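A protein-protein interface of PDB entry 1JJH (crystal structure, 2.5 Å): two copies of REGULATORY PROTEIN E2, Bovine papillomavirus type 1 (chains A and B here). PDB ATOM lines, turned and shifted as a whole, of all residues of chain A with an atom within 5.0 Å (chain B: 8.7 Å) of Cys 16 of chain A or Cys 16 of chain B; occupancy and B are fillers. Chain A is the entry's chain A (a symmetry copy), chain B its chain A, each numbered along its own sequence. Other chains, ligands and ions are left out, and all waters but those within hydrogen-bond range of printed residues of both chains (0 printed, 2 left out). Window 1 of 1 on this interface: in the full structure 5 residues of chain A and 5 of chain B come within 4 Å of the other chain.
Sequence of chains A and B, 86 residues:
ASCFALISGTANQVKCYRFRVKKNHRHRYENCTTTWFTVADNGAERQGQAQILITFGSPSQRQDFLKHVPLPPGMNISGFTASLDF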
ATOM      1  N   ASN A  12      -8.339  -8.872 -32.847  1.00  0.00           N
ATOM      2  CA  ASN A  12      -7.155  -9.237 -32.074  1.00  0.00           C
ATOM      3  C   ASN A  12      -7.453  -9.774 -30.680  1.00  0.00           C
ATOM      4  O   ASN A  12      -6.834 -10.750 -30.244  1.00  0.00           O
ATOM      5  CB  ASN A  12      -6.212  -8.041 -31.975  1.00  0.00           C
ATOM      6  CG  ASN A  12      -5.163  -8.046 -33.053  1.00  0.00           C
ATOM      7  OD1 ASN A  12      -5.376  -8.566 -34.142  1.00  0.00           O
ATOM      8  ND2 ASN A  12      -4.023  -7.454 -32.761  1.00  0.00           N
ATOM      9  N   GLN A  13      -8.383  -9.127 -29.979  1.00  0.00           N
ATOM     10  CA  GLN A  13      -8.766  -9.572 -28.637  1.00  0.00           C
ATOM     11  C   GLN A  13      -9.283 -10.997 -28.742  1.00  0.00           C
ATOM     12  O   GLN A  13      -8.838 -11.898 -28.029  1.00  0.00           O
ATOM     13  CB  GLN A  13      -9.885  -8.697 -28.069  1.00  0.00           C
ATOM     14  CG  GLN A  13      -9.496  -7.262 -27.746  1.00  0.00           C
ATOM     15  CD  GLN A  13     -10.703  -6.410 -27.349  1.00  0.00           C
ATOM     16  OE1 GLN A  13     -11.572  -6.103 -28.174  1.00  0.00           O
ATOM     17  NE2 GLN A  13     -10.763  -6.034 -26.076  1.00  0.00           N
ATOM     18  N   VAL A  14     -10.228 -11.191 -29.656  1.00  0.00           N
ATOM     19  CA  VAL A  14     -10.839 -12.488 -29.874  1.00  0.00           C
ATOM     20  C   VAL A  14      -9.809 -13.541 -30.224  1.00  0.00           C
ATOM     21  O   VAL A  14      -9.780 -14.616 -29.621  1.00  0.00           O
ATOM     22  CB  VAL A  14     -11.931 -12.398 -30.968  1.00  0.00           C
ATOM     23  CG1 VAL A  14     -12.196 -13.759 -31.571  1.00  0.00           C
ATOM     24  CG2 VAL A  14     -13.226 -11.856 -30.343  1.00  0.00           C
ATOM     25  N   LYS A  15      -8.946 -13.235 -31.181  1.00  0.00           N
ATOM     26  CA  LYS A  15      -7.926 -14.200 -31.575  1.00  0.00           C
ATOM     27  C   LYS A  15      -6.976 -14.588 -30.439  1.00  0.00           C
ATOM     28  O   LYS A  15      -6.637 -15.764 -30.276  1.00  0.00           O
ATOM     29  CB  LYS A  15      -7.089 -13.664 -32.731  1.00  0.00           C
ATOM     30  CG  LYS A  15      -6.108 -14.700 -33.261  1.00  0.00           C
ATOM     31  CD  LYS A  15      -4.865 -14.069 -33.861  1.00  0.00           C
ATOM     32  CE  LYS A  15      -3.931 -15.142 -34.422  1.00  0.00           C
ATOM     33  NZ  LYS A  15      -3.549 -16.147 -33.380  1.00  0.00           N
ATOM     34  N   CYS A  16      -6.527 -13.615 -29.659  1.00  0.00           N
ATOM     35  CA  CYS A  16      -5.597 -13.935 -28.593  1.00  0.00           C
ATOM     36  C   CYS A  16      -6.242 -14.593 -27.401  1.00  0.00           C
ATOM     37  O   CYS A  16      -5.606 -15.378 -26.690  1.00  0.00           O
ATOM     38  CB  CYS A  16      -4.815 -12.690 -28.190  1.00  0.00           C
ATOM     39  SG  CYS A  16      -3.557 -12.328 -29.441  1.00  0.00           S
ATOM     40  N   TYR A  17      -7.509 -14.272 -27.181  1.00  0.00           N
ATOM     41  CA  TYR A  17      -8.266 -14.875 -26.101  1.00  0.00           C
ATOM     42  C   TYR A  17      -8.343 -16.376 -26.415  1.00  0.00           C
ATOM     43  O   TYR A  17      -7.993 -17.220 -25.585  1.00  0.00           O
ATOM     44  CB  TYR A  17      -9.659 -14.239 -26.061  1.00  0.00           C
ATOM     45  CG  TYR A  17     -10.632 -14.892 -25.117  1.00  0.00           C
ATOM     46  CD1 TYR A  17     -11.418 -15.972 -25.531  1.00  0.00           C
ATOM     47  CD2 TYR A  17     -10.762 -14.438 -23.804  1.00  0.00           C
ATOM     48  CE1 TYR A  17     -12.306 -16.583 -24.661  1.00  0.00           C
ATOM     49  CE2 TYR A  17     -11.649 -15.045 -22.922  1.00  0.00           C
ATOM     50  CZ  TYR A  17     -12.419 -16.114 -23.355  1.00  0.00           C
ATOM     51  OH  TYR A  17     -13.311 -16.705 -22.487  1.00  0.00           O
ATOM     52  N   ARG A  18      -8.776 -16.704 -27.629  1.00  0.00           N
ATOM     53  CA  ARG A  18      -8.885 -18.099 -28.041  1.00  0.00           C
ATOM     54  C   ARG A  18      -7.560 -18.836 -27.873  1.00  0.00           C
ATOM     55  O   ARG A  18      -7.515 -19.960 -27.369  1.00  0.00           O
ATOM     56  CB  ARG A  18      -9.343 -18.197 -29.497  1.00  0.00           C
ATOM     57  CG  ARG A  18      -9.544 -19.623 -29.956  1.00  0.00           C
ATOM     58  CD  ARG A  18     -10.001 -19.679 -31.401  1.00  0.00           C
ATOM     59  NE  ARG A  18      -9.047 -19.038 -32.300  1.00  0.00           N
ATOM     60  CZ  ARG A  18      -9.376 -18.107 -33.194  1.00  0.00           C
ATOM     61  NH1 ARG A  18     -10.641 -17.713 -33.307  1.00  0.00           N
ATOM     62  NH2 ARG A  18      -8.439 -17.561 -33.965  1.00  0.00           N
ATOM     63  N   PHE A  19      -6.484 -18.193 -28.304  1.00  0.00           N
ATOM     64  CA  PHE A  19      -5.155 -18.762 -28.205  1.00  0.00           C
ATOM     65  C   PHE A  19      -4.791 -19.085 -26.753  1.00  0.00           C
ATOM     66  O   PHE A  19      -4.191 -20.125 -26.472  1.00  0.00           O
ATOM     67  CB  PHE A  19      -4.153 -17.784 -28.820  1.00  0.00           C
ATOM     68  CG  PHE A  19      -2.719 -18.165 -28.606  1.00  0.00           C
ATOM     69  CD1 PHE A  19      -2.011 -17.683 -27.495  1.00  0.00           C
ATOM     70  CD2 PHE A  19      -2.076 -19.020 -29.495  1.00  0.00           C
ATOM     71  CE1 PHE A  19      -0.688 -18.050 -27.280  1.00  0.00           C
ATOM     72  CE2 PHE A  19      -0.752 -19.394 -29.288  1.00  0.00           C
ATOM     73  CZ  PHE A  19      -0.056 -18.909 -28.181  1.00  0.00           C
ATOM     74  N   ARG A  20      -5.166 -18.193 -25.836  1.00  0.00           N
ATOM     75  CA  ARG A  20      -4.890 -18.352 -24.407  1.00  0.00           C
ATOM     76  C   ARG A  20      -5.676 -19.531 -23.844  1.00  0.00           C
ATOM     77  O   ARG A  20      -5.119 -20.422 -23.188  1.00  0.00           O
ATOM     78  CB  ARG A  20      -5.292 -17.080 -23.656  1.00  0.00           C
ATOM     79  CG  ARG A  20      -4.139 -16.310 -23.018  1.00  0.00           C
ATOM     80  CD  ARG A  20      -4.624 -14.994 -22.389  1.00  0.00           C
ATOM     81  NE  ARG A  20      -4.766 -13.913 -23.370  1.00  0.00           N
ATOM     82  CZ  ARG A  20      -5.901 -13.272 -23.640  1.00  0.00           C
ATOM     83  NH1 ARG A  20      -7.022 -13.597 -23.008  1.00  0.00           N
ATOM     84  NH2 ARG A  20      -5.913 -12.297 -24.537  1.00  0.00           N
ATOM     85  N   THR B  10       6.175 -19.486 -32.375  1.00  0.00           N
ATOM     86  CA  THR B  10       5.204 -19.784 -33.422  1.00  0.00           C
ATOM     87  C   THR B  10       4.552 -18.473 -33.851  1.00  0.00           C
ATOM     88  O   THR B  10       4.635 -17.472 -33.138  1.00  0.00           O
ATOM     89  CB  THR B  10       4.123 -20.758 -32.927  1.00  0.00           C
ATOM     90  OG1 THR B  10       3.417 -20.167 -31.834  1.00  0.00           O
ATOM     91  CG2 THR B  10       4.754 -22.058 -32.465  1.00  0.00           C
ATOM     92  N   ALA B  11       3.924 -18.474 -35.021  1.00  0.00           N
ATOM     93  CA  ALA B  11       3.273 -17.272 -35.528  1.00  0.00           C
ATOM     94  C   ALA B  11       2.274 -16.725 -34.504  1.00  0.00           C
ATOM     95  O   ALA B  11       2.178 -15.507 -34.303  1.00  0.00           O
ATOM     96  CB  ALA B  11       2.569 -17.579 -36.838  1.00  0.00           C
ATOM     97  N   ASN B  12       1.546 -17.631 -33.854  1.00  0.00           N
ATOM     98  CA  ASN B  12       0.546 -17.261 -32.856  1.00  0.00           C
ATOM     99  C   ASN B  12       1.123 -16.720 -31.556  1.00  0.00           C
ATOM    100  O   ASN B  12       0.606 -15.742 -31.006  1.00  0.00           O
ATOM    101  CB  ASN B  12      -0.356 -18.457 -32.561  1.00  0.00           C
ATOM    102  CG  ASN B  12      -1.604 -18.456 -33.403  1.00  0.00           C
ATOM    103  OD1 ASN B  12      -1.619 -17.940 -34.512  1.00  0.00           O
ATOM    104  ND2 ASN B  12      -2.660 -19.047 -32.880  1.00  0.00           N
ATOM    105  N   GLN B  13       2.178 -17.364 -31.057  1.00  0.00           N
ATOM    106  CA  GLN B  13       2.827 -16.914 -29.824  1.00  0.00           C
ATOM    107  C   GLN B  13       3.311 -15.490 -30.039  1.00  0.00           C
ATOM    108  O   GLN B  13       3.022 -14.586 -29.252  1.00  0.00           O
ATOM    109  CB  GLN B  13       4.039 -17.788 -29.494  1.00  0.00           C
ATOM    110  CG  GLN B  13       3.725 -19.222 -29.094  1.00  0.00           C
ATOM    111  CD  GLN B  13       4.988 -20.072 -28.948  1.00  0.00           C
ATOM    112  OE1 GLN B  13       5.670 -20.382 -29.934  1.00  0.00           O
ATOM    113  NE2 GLN B  13       5.307 -20.444 -27.714  1.00  0.00           N
ATOM    114  N   VAL B  14       4.048 -15.300 -31.127  1.00  0.00           N
ATOM    115  CA  VAL B  14       4.601 -14.004 -31.470  1.00  0.00           C
ATOM    116  C   VAL B  14       3.521 -12.952 -31.607  1.00  0.00           C
ATOM    117  O   VAL B  14       3.617 -11.874 -31.014  1.00  0.00           O
ATOM    118  CB  VAL B  14       5.446 -14.099 -32.765  1.00  0.00           C
ATOM    119  CG1 VAL B  14       5.581 -12.740 -33.414  1.00  0.00           C
ATOM    120  CG2 VAL B  14       6.842 -14.639 -32.417  1.00  0.00           C
ATOM    121  N   LYS B  15       2.480 -13.262 -32.365  1.00  0.00           N
ATOM    122  CA  LYS B  15       1.401 -12.297 -32.545  1.00  0.00           C
ATOM    123  C   LYS B  15       0.704 -11.905 -31.239  1.00  0.00           C
ATOM    124  O   LYS B  15       0.405 -10.729 -31.015  1.00  0.00           O
ATOM    125  CB  LYS B  15       0.344 -12.838 -33.503  1.00  0.00           C
ATOM    126  CG  LYS B  15      -0.725 -11.803 -33.824  1.00  0.00           C
ATOM    127  CD  LYS B  15      -2.063 -12.436 -34.154  1.00  0.00           C
ATOM    128  CE  LYS B  15      -3.093 -11.364 -34.516  1.00  0.00           C
ATOM    129  NZ  LYS B  15      -3.253 -10.355 -33.422  1.00  0.00           N
ATOM    130  N   CYS B  16       0.425 -12.874 -30.381  1.00  0.00           N
ATOM    131  CA  CYS B  16      -0.268 -12.551 -29.148  1.00  0.00           C
ATOM    132  C   CYS B  16       0.608 -11.888 -28.116  1.00  0.00           C
ATOM    133  O   CYS B  16       0.131 -11.100 -27.292  1.00  0.00           O
ATOM    134  CB  CYS B  16      -0.950 -13.794 -28.588  1.00  0.00           C
ATOM    135  SG  CYS B  16      -2.438 -14.160 -29.553  1.00  0.00           S
ATOM    136  N   TYR B  17       1.893 -12.209 -28.159  1.00  0.00           N
ATOM    137  CA  TYR B  17       2.855 -11.602 -27.260  1.00  0.00           C
ATOM    138  C   TYR B  17       2.866 -10.102 -27.588  1.00  0.00           C
ATOM    139  O   TYR B  17       2.692  -9.255 -26.707  1.00  0.00           O
ATOM    140  CB  TYR B  17       4.227 -12.239 -27.504  1.00  0.00           C
ATOM    141  CG  TYR B  17       5.373 -11.582 -26.782  1.00  0.00           C
ATOM    142  CD1 TYR B  17       6.057 -10.504 -27.351  1.00  0.00           C
ATOM    143  CD2 TYR B  17       5.770 -12.031 -25.522  1.00  0.00           C
ATOM    144  CE1 TYR B  17       7.105  -9.890 -26.684  1.00  0.00           C
ATOM    145  CE2 TYR B  17       6.818 -11.421 -24.842  1.00  0.00           C
ATOM    146  CZ  TYR B  17       7.483 -10.354 -25.428  1.00  0.00           C
ATOM    147  OH  TYR B  17       8.533  -9.760 -24.763  1.00  0.00           O
ATOM    148  N   ARG B  18       3.041  -9.779 -28.866  1.00  0.00           N
ATOM    149  CA  ARG B  18       3.063  -8.386 -29.296  1.00  0.00           C
ATOM    150  C   ARG B  18       1.799  -7.648 -28.863  1.00  0.00           C
ATOM    151  O   ARG B  18       1.858  -6.521 -28.366  1.00  0.00           O
ATOM    152  CB  ARG B  18       3.212  -8.293 -30.816  1.00  0.00           C
ATOM    153  CG  ARG B  18       3.314  -6.869 -31.312  1.00  0.00           C
ATOM    154  CD  ARG B  18       3.466  -6.818 -32.821  1.00  0.00           C
ATOM    155  NE  ARG B  18       2.348  -7.463 -33.503  1.00  0.00           N
ATOM    156  CZ  ARG B  18       2.487  -8.397 -34.442  1.00  0.00           C
ATOM    157  NH1 ARG B  18       3.702  -8.792 -34.809  1.00  0.00           N
ATOM    158  NH2 ARG B  18       1.411  -8.946 -35.002  1.00  0.00           N
ATOM    159  N   PHE B  19       0.658  -8.292 -29.063  1.00  0.00           N
ATOM    160  CA  PHE B  19      -0.622  -7.722 -28.695  1.00  0.00           C
ATOM    161  C   PHE B  19      -0.681  -7.393 -27.200  1.00  0.00           C
ATOM    162  O   PHE B  19      -1.211  -6.351 -26.806  1.00  0.00           O
ATOM    163  CB  PHE B  19      -1.729  -8.702 -29.088  1.00  0.00           C
ATOM    164  CG  PHE B  19      -3.088  -8.319 -28.586  1.00  0.00           C
ATOM    165  CD1 PHE B  19      -3.553  -8.797 -27.352  1.00  0.00           C
ATOM    166  CD2 PHE B  19      -3.900  -7.467 -29.328  1.00  0.00           C
ATOM    167  CE1 PHE B  19      -4.804  -8.429 -26.872  1.00  0.00           C
ATOM    168  CE2 PHE B  19      -5.154  -7.092 -28.855  1.00  0.00           C
ATOM    169  CZ  PHE B  19      -5.609  -7.572 -27.628  1.00  0.00           C
ATOM    170  N   ARG B  20      -0.126  -8.282 -26.377  1.00  0.00           N
ATOM    171  CA  ARG B  20      -0.103  -8.117 -24.922  1.00  0.00           C
ATOM    172  C   ARG B  20       0.781  -6.936 -24.537  1.00  0.00           C
ATOM    173  O   ARG B  20       0.370  -6.043 -23.784  1.00  0.00           O
ATOM    174  CB  ARG B  20       0.445  -9.387 -24.265  1.00  0.00           C
ATOM    175  CG  ARG B  20      -0.552 -10.154 -23.401  1.00  0.00           C
ATOM    176  CD  ARG B  20       0.051 -11.468 -22.879  1.00  0.00           C
ATOM    177  NE  ARG B  20      -0.010 -12.553 -23.865  1.00  0.00           N
ATOM    178  CZ  ARG B  20       1.047 -13.194 -24.360  1.00  0.00           C
ATOM    179  NH1 ARG B  20       2.272 -12.868 -23.972  1.00  0.00           N
ATOM    180  NH2 ARG B  20       0.875 -14.172 -25.237  1.00  0.00           N
ATOM    181  N   VAL B  21       2.004  -6.951 -25.065  1.00  0.00           N
ATOM    182  CA  VAL B  21       2.996  -5.919 -24.816  1.00  0.00           C
ATOM    183  C   VAL B  21       2.503  -4.550 -25.267  1.00  0.00           C
ATOM    184  O   VAL B  21       2.788  -3.533 -24.634  1.00  0.00           O
ATOM    185  CB  VAL B  21       4.324  -6.289 -25.524  1.00  0.00           C
ATOM    186  CG1 VAL B  21       5.251  -5.081 -25.633  1.00  0.00           C
ATOM    187  CG2 VAL B  21       5.011  -7.388 -24.726  1.00  0.00           C
ATOM    188  N   LYS B  22       1.741  -4.530 -26.350  1.00  0.00           N
ATOM    189  CA  LYS B  22       1.213  -3.275 -26.868  1.00  0.00           C
ATOM    190  C   LYS B  22       0.047  -2.715 -26.046  1.00  0.00           C
ATOM    191  O   LYS B  22      -0.040  -1.513 -25.830  1.00  0.00           O
ATOM    192  CB  LYS B  22       0.778  -3.464 -28.320  1.00  0.00           C
ATOM    193  CG  LYS B  22       0.198  -2.223 -28.956  1.00  0.00           C
ATOM    194  CD  LYS B  22      -0.370  -2.562 -30.309  1.00  0.00           C
ATOM    195  CE  LYS B  22      -1.193  -1.427 -30.861  1.00  0.00           C
ATOM    196  NZ  LYS B  22      -1.758  -1.812 -32.179  1.00  0.00           N
ATOM    197  N   LYS B  23      -0.853  -3.579 -25.590  1.00  0.00           N
ATOM    198  CA  LYS B  23      -1.994  -3.116 -24.811  1.00  0.00           C
ATOM    199  C   LYS B  23      -1.672  -2.907 -23.333  1.00  0.00           C
ATOM    200  O   LYS B  23      -2.261  -2.053 -22.680  1.00  0.00           O
ATOM    201  CB  LYS B  23      -3.164  -4.102 -24.945  1.00  0.00           C
ATOM    202  CG  LYS B  23      -3.701  -4.226 -26.367  1.00  0.00           C
ATOM    203  CD  LYS B  23      -4.220  -2.887 -26.906  1.00  0.00           C
ATOM    204  CE  LYS B  23      -4.679  -3.007 -28.353  1.00  0.00           C
ATOM    205  NZ  LYS B  23      -5.384  -1.783 -28.832  1.00  0.00           N
ATOM    206  N   ASN B  24      -0.732  -3.679 -22.808  1.00  0.00           N
ATOM    207  CA  ASN B  24      -0.390  -3.563 -21.400  1.00  0.00           C
ATOM    208  C   ASN B  24       0.972  -2.944 -21.077  1.00  0.00           C
ATOM    209  O   ASN B  24       1.160  -2.475 -19.964  1.00  0.00           O
ATOM    210  CB  ASN B  24      -0.495  -4.943 -20.736  1.00  0.00           C
ATOM    211  CG  ASN B  24      -1.864  -5.595 -20.941  1.00  0.00           C
ATOM    212  OD1 ASN B  24      -1.975  -6.819 -21.016  1.00  0.00           O
ATOM    213  ND2 ASN B  24      -2.910  -4.775 -21.019  1.00  0.00           N
ATOM    214  N   THR B  35       4.939  -9.301 -37.676  1.00  0.00           N
ATOM    215  CA  THR B  35       5.619 -10.592 -37.758  1.00  0.00           C
ATOM    216  C   THR B  35       6.344 -10.826 -39.086  1.00  0.00           C
ATOM    217  O   THR B  35       5.836 -10.491 -40.166  1.00  0.00           O
ATOM    218  CB  THR B  35       4.615 -11.731 -37.559  1.00  0.00           C
ATOM    219  OG1 THR B  35       3.951 -11.555 -36.301  1.00  0.00           O
ATOM    220  CG2 THR B  35       5.314 -13.082 -37.583  1.00  0.00           C
ATOM    221  N   ALA B  50       8.325 -17.574 -36.241  1.00  0.00           N
ATOM    222  CA  ALA B  50       7.897 -16.187 -36.325  1.00  0.00           C
ATOM    223  C   ALA B  50       8.923 -15.314 -35.604  1.00  0.00           C
ATOM    224  O   ALA B  50       9.582 -15.758 -34.666  1.00  0.00           O
ATOM    225  CB  ALA B  50       6.513 -16.020 -35.703  1.00  0.00           C
ATOM    226  N   ILE B  52       9.710 -11.027 -34.343  1.00  0.00           N
ATOM    227  CA  ILE B  52       9.334  -9.625 -34.247  1.00  0.00           C
ATOM    228  C   ILE B  52      10.513  -8.906 -33.632  1.00  0.00           C
ATOM    229  O   ILE B  52      11.271  -9.481 -32.839  1.00  0.00           O
ATOM    230  CB  ILE B  52       8.080  -9.361 -33.392  1.00  0.00           C
ATOM    231  CG1 ILE B  52       8.240  -9.946 -31.987  1.00  0.00           C
ATOM    232  CG2 ILE B  52       6.866  -9.901 -34.099  1.00  0.00           C
ATOM    233  CD1 ILE B  52       7.116  -9.537 -31.037  1.00  0.00           C
ATOM    234  N   PRO B  72       6.871 -16.143 -22.415  1.00  0.00           N
ATOM    235  CA  PRO B  72       6.065 -17.371 -22.406  1.00  0.00           C
ATOM    236  C   PRO B  72       6.861 -18.622 -22.799  1.00  0.00           C
ATOM    237  O   PRO B  72       7.765 -18.565 -23.642  1.00  0.00           O
ATOM    238  CB  PRO B  72       4.951 -17.063 -23.409  1.00  0.00           C
ATOM    239  CG  PRO B  72       4.806 -15.577 -23.309  1.00  0.00           C
ATOM    240  CD  PRO B  72       6.248 -15.122 -23.280  1.00  0.00           C
ATOM    241  N   MET B  75       8.992 -19.712 -26.129  1.00  0.00           N
ATOM    242  CA  MET B  75       9.434 -18.523 -26.853  1.00  0.00           C
ATOM    243  C   MET B  75      10.885 -18.136 -26.555  1.00  0.00           C
ATOM    244  O   MET B  75      11.436 -18.497 -25.515  1.00  0.00           O
ATOM    245  CB  MET B  75       8.501 -17.352 -26.545  1.00  0.00           C
ATOM    246  CG  MET B  75       7.054 -17.655 -26.890  1.00  0.00           C
ATOM    247  SD  MET B  75       6.026 -16.188 -26.940  1.00  0.00           S
ATOM    248  CE  MET B  75       6.617 -15.446 -28.473  1.00  0.00           C
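The side-chain sulfur (SG) of Cys 16 of chain B is disulfide-bonded to the side-chain sulfur (SG) of Cys 16 of chain A (2.1 Å). OD1 of Asn 12 of chain B sits at hydrogen-bond distance from NZ of Lys 15 of chain A (2.9 Å). The side-chain amide oxygen (OD1) of Asn 12 of chain A sits at hydrogen-bond distance from the side-chain amino group (NZ) of Lys 15 of chain B, 2.9 Å away.
Of the 20 printed residues of chain B, 5 touch a printed residue of chain A. Hydrophobic or aromatic side chains of chain B that line the printed part of chain A: Phe 19. Hydrophobic or aromatic side chains of chain A that line the printed part of chain B: Phe 19. Among the printed residues, 8 pairs touch across the chains.
Asn 12 of chain A touches Lys 15 of chain B, and with the chains exchanged Lys 15 of chain A touches Asn 12 of chain B. Asn 12 of chain A touches Phe 19 of chain B, and with the chains exchanged Phe 19 of chain A touches Asn 12 of chain B. Lys 15 of chain B touches its own counterpart, Lys 15 of chain A. Cys 16 of chain B touches its own counterpart, Cys 16 of chain A. Of the 8 pairs that touch across the chains among the printed residues, 8 have their exchanged pair printed and touching as well.
CE2 of Phe 19 of chain B touches CB of Asn 12 of chain A, at 3.4 Å. Phe 19 of chain B touches Gln 13 of chain A (CZ to CA, 3.9 Å). Lys 15 of chain B touches Lys 15 of chain A (CD to CD, 3.3 Å). CB of Asn 12 of chain B touches CE2 of Phe 19 of chain A, at 3.4 Å. CZ of Phe 19 of chain A touches CA of Gln 13 of chain B, at 3.9 Å.
OE1 of Gln 13 of chain B is in hydrogen-bond range of N of Thr 10 of chain B (2.6 Å).
Cys 16 of chain A touches just one residue of chain B: Cys 16. Printed residues of chain B within 4 Å of Phe 19 of chain A: Asn 12 and Gln 13. Printed residues of chain A within 4 Å of Asn 12 of chain B: Lys 15 and Phe 19. Printed residues of chain A within 4 Å of Cys 16 of chain B: Cys 16. Met 75 of chain B touches none of the printed residues of chain A. The nearest residue of chain B that does not touch Cys 16 of chain A is Phe 19 of chain B (4.1 Å). The nearest printed residue of chain A that does not touch Phe 19 of chain B is Cys 16 of chain A (4.1 Å).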
